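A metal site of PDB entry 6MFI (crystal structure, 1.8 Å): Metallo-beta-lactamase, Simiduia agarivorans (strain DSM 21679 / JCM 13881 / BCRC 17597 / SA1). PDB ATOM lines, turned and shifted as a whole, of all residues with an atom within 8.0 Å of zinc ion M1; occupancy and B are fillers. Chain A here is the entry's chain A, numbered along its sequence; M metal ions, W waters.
OD2 of Asp 149 sits at hydrogen-bond distance from NE2 of His 112 (2.9 Å).
The side-chain carboxylate (OD1) of Asp 212 is in hydrogen-bond range of a ring nitrogen (ND1) of His 110, 2.5 Å away.
A ring nitrogen (ND1) of His 188 sits at hydrogen-bond distance from the side-chain hydroxyl (OG) of Ser 215.
Within 4 Å of zinc ion M1: His 110, His 112 and His 188.
Zinc ion M1 is bound by water W1 (2.0 Å), a ring nitrogen (ND1) of His 112 (2.0 Å), a ring nitrogen (NE2) of His 188 (2.0 Å) and a ring nitrogen (NE2) of His 110 (2.2 Å).
Zinc ion M1 has four donor atoms within binding distance.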
ATOM      1  N   TRP A  43     -15.050  20.836   3.598  1.00  0.00           N
ATOM      2  CA  TRP A  43     -13.718  20.256   3.742  1.00  0.00           C
ATOM      3  C   TRP A  43     -12.801  21.136   4.580  1.00  0.00           C
ATOM      4  O   TRP A  43     -12.000  20.632   5.368  1.00  0.00           O
ATOM      5  CB  TRP A  43     -13.102  20.012   2.367  1.00  0.00           C
ATOM      6  CG  TRP A  43     -13.766  18.926   1.574  1.00  0.00           C
ATOM      7  CD1 TRP A  43     -14.644  17.985   2.052  1.00  0.00           C
ATOM      8  CD2 TRP A  43     -13.615  18.663   0.183  1.00  0.00           C
ATOM      9  NE1 TRP A  43     -15.044  17.155   1.034  1.00  0.00           N
ATOM     10  CE2 TRP A  43     -14.425  17.554  -0.125  1.00  0.00           C
ATOM     11  CE3 TRP A  43     -12.884  19.260  -0.842  1.00  0.00           C
ATOM     12  CZ2 TRP A  43     -14.510  17.023  -1.415  1.00  0.00           C
ATOM     13  CZ3 TRP A  43     -12.972  18.733  -2.124  1.00  0.00           C
ATOM     14  CH2 TRP A  43     -13.785  17.631  -2.401  1.00  0.00           C
ATOM     15  N   SER A 109      -4.116   8.557   2.998  1.00  0.00           N
ATOM     16  CA  SER A 109      -5.162   7.630   2.581  1.00  0.00           C
ATOM     17  C   SER A 109      -5.085   7.449   1.063  1.00  0.00           C
ATOM     18  O   SER A 109      -4.623   6.409   0.583  1.00  0.00           O
ATOM     19  CB  SER A 109      -6.540   8.147   2.991  1.00  0.00           C
ATOM     20  OG  SER A 109      -6.777   9.449   2.499  1.00  0.00           O
ATOM     21  N   HIS A 110      -5.543   8.453   0.315  1.00  0.00           N
ATOM     22  CA  HIS A 110      -5.389   8.459  -1.136  1.00  0.00           C
ATOM     23  C   HIS A 110      -5.013   9.860  -1.595  1.00  0.00           C
ATOM     24  O   HIS A 110      -5.195  10.842  -0.874  1.00  0.00           O
ATOM     25  CB  HIS A 110      -6.645   7.948  -1.848  1.00  0.00           C
ATOM     26  CG  HIS A 110      -7.857   8.797  -1.631  1.00  0.00           C
ATOM     27  ND1 HIS A 110      -8.814   8.491  -0.682  1.00  0.00           N
ATOM     28  CD2 HIS A 110      -8.292   9.919  -2.252  1.00  0.00           C
ATOM     29  CE1 HIS A 110      -9.771   9.398  -0.714  1.00  0.00           C
ATOM     30  NE2 HIS A 110      -9.482  10.265  -1.663  1.00  0.00           N
ATOM     31  N   GLU A 111      -4.496   9.937  -2.812  1.00  0.00           N
ATOM     32  CA  GLU A 111      -3.795  11.121  -3.324  1.00  0.00           C
ATOM     33  C   GLU A 111      -4.718  12.164  -3.927  1.00  0.00           C
ATOM     34  O   GLU A 111      -4.391  12.765  -4.956  1.00  0.00           O
ATOM     35  CB  GLU A 111      -2.742  10.678  -4.341  1.00  0.00           C
ATOM     36  CG  GLU A 111      -3.301   9.858  -5.507  1.00  0.00           C
ATOM     37  CD  GLU A 111      -3.382   8.365  -5.208  1.00  0.00           C
ATOM     38  OE1 GLU A 111      -3.233   7.572  -6.152  1.00  0.00           O
ATOM     39  OE2 GLU A 111      -3.610   8.006  -4.037  1.00  0.00           O
ATOM     40  N   HIS A 112      -5.871  12.429  -3.320  1.00  0.00           N
ATOM     41  CA  HIS A 112      -6.747  13.491  -3.786  1.00  0.00           C
ATOM     42  C   HIS A 112      -6.467  14.779  -3.003  1.00  0.00           C
ATOM     43  O   HIS A 112      -5.983  14.742  -1.870  1.00  0.00           O
ATOM     44  CB  HIS A 112      -8.207  13.093  -3.655  1.00  0.00           C
ATOM     45  CG  HIS A 112      -8.719  12.283  -4.807  1.00  0.00           C
ATOM     46  ND1 HIS A 112     -10.035  11.860  -4.891  1.00  0.00           N
ATOM     47  CD2 HIS A 112      -8.094  11.819  -5.907  1.00  0.00           C
ATOM     48  CE1 HIS A 112     -10.191  11.170  -6.013  1.00  0.00           C
ATOM     49  NE2 HIS A 112      -9.035  11.134  -6.648  1.00  0.00           N
ATOM     50  N   ILE A 113      -6.784  15.906  -3.640  1.00  0.00           N
ATOM     51  CA  ILE A 113      -6.387  17.210  -3.090  1.00  0.00           C
ATOM     52  C   ILE A 113      -7.055  17.477  -1.746  1.00  0.00           C
ATOM     53  O   ILE A 113      -6.486  18.172  -0.904  1.00  0.00           O
ATOM     54  CB  ILE A 113      -6.711  18.326  -4.113  1.00  0.00           C
ATOM     55  CG1 ILE A 113      -6.215  19.683  -3.599  1.00  0.00           C
ATOM     56  CG2 ILE A 113      -8.198  18.371  -4.420  1.00  0.00           C
ATOM     57  CD1 ILE A 113      -6.542  20.841  -4.514  1.00  0.00           C
ATOM     58  N   ASP A 114      -8.246  16.920  -1.516  1.00  0.00           N
ATOM     59  CA  ASP A 114      -8.929  17.180  -0.257  1.00  0.00           C
ATOM     60  C   ASP A 114      -8.319  16.416   0.915  1.00  0.00           C
ATOM     61  O   ASP A 114      -8.731  16.629   2.054  1.00  0.00           O
ATOM     62  CB  ASP A 114     -10.418  16.836  -0.374  1.00  0.00           C
ATOM     63  CG  ASP A 114     -10.661  15.432  -0.874  1.00  0.00           C
ATOM     64  OD1 ASP A 114      -9.970  15.012  -1.829  1.00  0.00           O
ATOM     65  OD2 ASP A 114     -11.538  14.744  -0.319  1.00  0.00           O
ATOM     66  N   HIS A 115      -7.356  15.536   0.665  1.00  0.00           N
ATOM     67  CA  HIS A 115      -6.715  14.758   1.726  1.00  0.00           C
ATOM     68  C   HIS A 115      -5.212  14.970   1.831  1.00  0.00           C
ATOM     69  O   HIS A 115      -4.663  14.847   2.925  1.00  0.00           O
ATOM     70  CB  HIS A 115      -6.983  13.261   1.532  1.00  0.00           C
ATOM     71  CG  HIS A 115      -8.444  12.921   1.482  1.00  0.00           C
ATOM     72  ND1 HIS A 115      -9.295  13.110   2.548  1.00  0.00           N
ATOM     73  CD2 HIS A 115      -9.208  12.404   0.478  1.00  0.00           C
ATOM     74  CE1 HIS A 115     -10.511  12.721   2.215  1.00  0.00           C
ATOM     75  NE2 HIS A 115     -10.481  12.291   0.965  1.00  0.00           N
ATOM     76  N   ASP A 149      -6.251   7.930 -12.574  1.00  0.00           N
ATOM     77  CA  ASP A 149      -7.085   8.410 -11.480  1.00  0.00           C
ATOM     78  C   ASP A 149      -8.521   8.561 -11.972  1.00  0.00           C
ATOM     79  O   ASP A 149      -8.755   9.233 -12.978  1.00  0.00           O
ATOM     80  CB  ASP A 149      -6.558   9.737 -10.939  1.00  0.00           C
ATOM     81  CG  ASP A 149      -6.997  10.001  -9.518  1.00  0.00           C
ATOM     82  OD1 ASP A 149      -6.147   9.908  -8.606  1.00  0.00           O
ATOM     83  OD2 ASP A 149      -8.194  10.294  -9.306  1.00  0.00           O
ATOM     84  N   GLN A 151     -10.898  10.393 -10.928  1.00  0.00           N
ATOM     85  CA  GLN A 151     -11.323  11.779 -10.897  1.00  0.00           C
ATOM     86  C   GLN A 151     -10.301  12.712 -11.551  1.00  0.00           C
ATOM     87  O   GLN A 151     -10.165  13.871 -11.149  1.00  0.00           O
ATOM     88  CB  GLN A 151     -11.598  12.220  -9.464  1.00  0.00           C
ATOM     89  CG  GLN A 151     -12.671  13.281  -9.322  1.00  0.00           C
ATOM     90  CD  GLN A 151     -12.967  13.629  -7.875  1.00  0.00           C
ATOM     91  OE1 GLN A 151     -13.003  12.764  -7.007  1.00  0.00           O
ATOM     92  NE2 GLN A 151     -13.171  14.918  -7.619  1.00  0.00           N
ATOM     93  N   HIS A 188     -10.788   3.912  -5.680  1.00  0.00           N
ATOM     94  CA  HIS A 188     -11.028   5.350  -5.651  1.00  0.00           C
ATOM     95  C   HIS A 188      -9.867   6.108  -6.285  1.00  0.00           C
ATOM     96  O   HIS A 188     -10.087   7.065  -7.037  1.00  0.00           O
ATOM     97  CB  HIS A 188     -11.249   5.808  -4.206  1.00  0.00           C
ATOM     98  CG  HIS A 188     -11.622   7.249  -4.076  1.00  0.00           C
ATOM     99  ND1 HIS A 188     -12.903   7.711  -4.297  1.00  0.00           N
ATOM    100  CD2 HIS A 188     -10.881   8.330  -3.758  1.00  0.00           C
ATOM    101  CE1 HIS A 188     -12.940   9.021  -4.116  1.00  0.00           C
ATOM    102  NE2 HIS A 188     -11.723   9.422  -3.789  1.00  0.00           N
ATOM    103  N   THR A 189      -8.643   5.698  -5.994  1.00  0.00           N
ATOM    104  CA  THR A 189      -7.436   6.175  -6.637  1.00  0.00           C
ATOM    105  C   THR A 189      -6.532   4.977  -6.895  1.00  0.00           C
ATOM    106  O   THR A 189      -6.700   3.926  -6.257  1.00  0.00           O
ATOM    107  CB  THR A 189      -6.682   7.201  -5.768  1.00  0.00           C
ATOM    108  OG1 THR A 189      -6.150   6.547  -4.610  1.00  0.00           O
ATOM    109  CG2 THR A 189      -7.589   8.343  -5.343  1.00  0.00           C
ATOM    110  N   ASP A 212      -9.694   3.607   3.489  1.00  0.00           N
ATOM    111  CA  ASP A 212      -9.798   4.637   2.475  1.00  0.00           C
ATOM    112  C   ASP A 212     -11.259   4.849   2.061  1.00  0.00           C
ATOM    113  O   ASP A 212     -12.144   4.047   2.362  1.00  0.00           O
ATOM    114  CB  ASP A 212      -8.939   4.266   1.266  1.00  0.00           C
ATOM    115  CG  ASP A 212      -8.844   5.392   0.246  1.00  0.00           C
ATOM    116  OD1 ASP A 212      -8.198   6.412   0.547  1.00  0.00           O
ATOM    117  OD2 ASP A 212      -9.418   5.249  -0.856  1.00  0.00           O
ATOM    118  N   SER A 213     -11.498   5.962   1.355  1.00  0.00           N
ATOM    119  CA  SER A 213     -12.845   6.283   0.896  1.00  0.00           C
ATOM    120  C   SER A 213     -13.425   5.149   0.064  1.00  0.00           C
ATOM    121  O   SER A 213     -14.591   4.766   0.253  1.00  0.00           O
ATOM    122  CB  SER A 213     -12.819   7.588   0.102  1.00  0.00           C
ATOM    123  OG  SER A 213     -12.291   8.642   0.883  1.00  0.00           O
ATOM    124  N   LEU A 214     -12.643   4.607  -0.868  1.00  0.00           N
ATOM    125  CA  LEU A 214     -13.010   3.440  -1.660  1.00  0.00           C
ATOM    126  C   LEU A 214     -14.260   3.669  -2.508  1.00  0.00           C
ATOM    127  O   LEU A 214     -14.764   2.722  -3.120  1.00  0.00           O
ATOM    128  CB  LEU A 214     -13.206   2.206  -0.779  1.00  0.00           C
ATOM    129  CG  LEU A 214     -11.966   1.699  -0.046  1.00  0.00           C
ATOM    130  CD1 LEU A 214     -12.244   0.373   0.615  1.00  0.00           C
ATOM    131  CD2 LEU A 214     -10.788   1.584  -0.987  1.00  0.00           C
ATOM    132  N   SER A 215     -14.760   4.908  -2.576  1.00  0.00           N
ATOM    133  CA  SER A 215     -16.014   5.184  -3.272  1.00  0.00           C
ATOM    134  C   SER A 215     -15.825   5.074  -4.781  1.00  0.00           C
ATOM    135  O   SER A 215     -14.845   5.595  -5.321  1.00  0.00           O
ATOM    136  CB  SER A 215     -16.525   6.572  -2.910  1.00  0.00           C
ATOM    137  OG  SER A 215     -15.512   7.542  -3.092  1.00  0.00           O
ATOM    138  N   VAL A 217     -16.609   6.733  -7.210  1.00  0.00           N
ATOM    139  CA  VAL A 217     -16.877   8.032  -7.783  1.00  0.00           C
ATOM    140  C   VAL A 217     -15.726   8.383  -8.716  1.00  0.00           C
ATOM    141  O   VAL A 217     -14.592   7.896  -8.563  1.00  0.00           O
ATOM    142  CB  VAL A 217     -17.074   9.121  -6.696  1.00  0.00           C
ATOM    143  CG1 VAL A 217     -15.739   9.497  -6.076  1.00  0.00           C
ATOM    144  CG2 VAL A 217     -17.790  10.341  -7.261  1.00  0.00           C
ATOM    145  N   PRO A 252     -11.375   8.891   5.947  1.00  0.00           N
ATOM    146  CA  PRO A 252     -10.942  10.257   5.610  1.00  0.00           C
ATOM    147  C   PRO A 252     -12.091  11.246   5.511  1.00  0.00           C
ATOM    148  O   PRO A 252     -11.926  12.415   5.873  1.00  0.00           O
ATOM    149  CB  PRO A 252     -10.237  10.067   4.253  1.00  0.00           C
ATOM    150  CG  PRO A 252      -9.827   8.640   4.249  1.00  0.00           C
ATOM    151  CD  PRO A 252     -10.903   7.901   4.976  1.00  0.00           C
ATOM    152  N   HIS A 253     -13.251  10.799   5.028  1.00  0.00           N
ATOM    153  CA  HIS A 253     -14.476  11.555   5.191  1.00  0.00           C
ATOM    154  C   HIS A 253     -15.203  10.983   6.393  1.00  0.00           C
ATOM    155  O   HIS A 253     -15.685   9.840   6.333  1.00  0.00           O
ATOM    156  CB  HIS A 253     -15.349  11.468   3.947  1.00  0.00           C
ATOM    157  CG  HIS A 253     -14.722  12.072   2.726  1.00  0.00           C
ATOM    158  ND1 HIS A 253     -14.783  13.426   2.452  1.00  0.00           N
ATOM    159  CD2 HIS A 253     -14.030  11.515   1.709  1.00  0.00           C
ATOM    160  CE1 HIS A 253     -14.151  13.668   1.328  1.00  0.00           C
ATOM    161  NE2 HIS A 253     -13.677  12.528   0.853  1.00  0.00           N
HETATM  162 ZN    ZN M   1     -10.829  11.140  -3.170  1.00  0.00          ZN
HETATM  163 ZN    ZN M   2     -12.081  12.796  -0.480  1.00  0.00          ZN
HETATM  164  O   HOH W   1     -11.879  12.648  -2.449  1.00  0.00           O
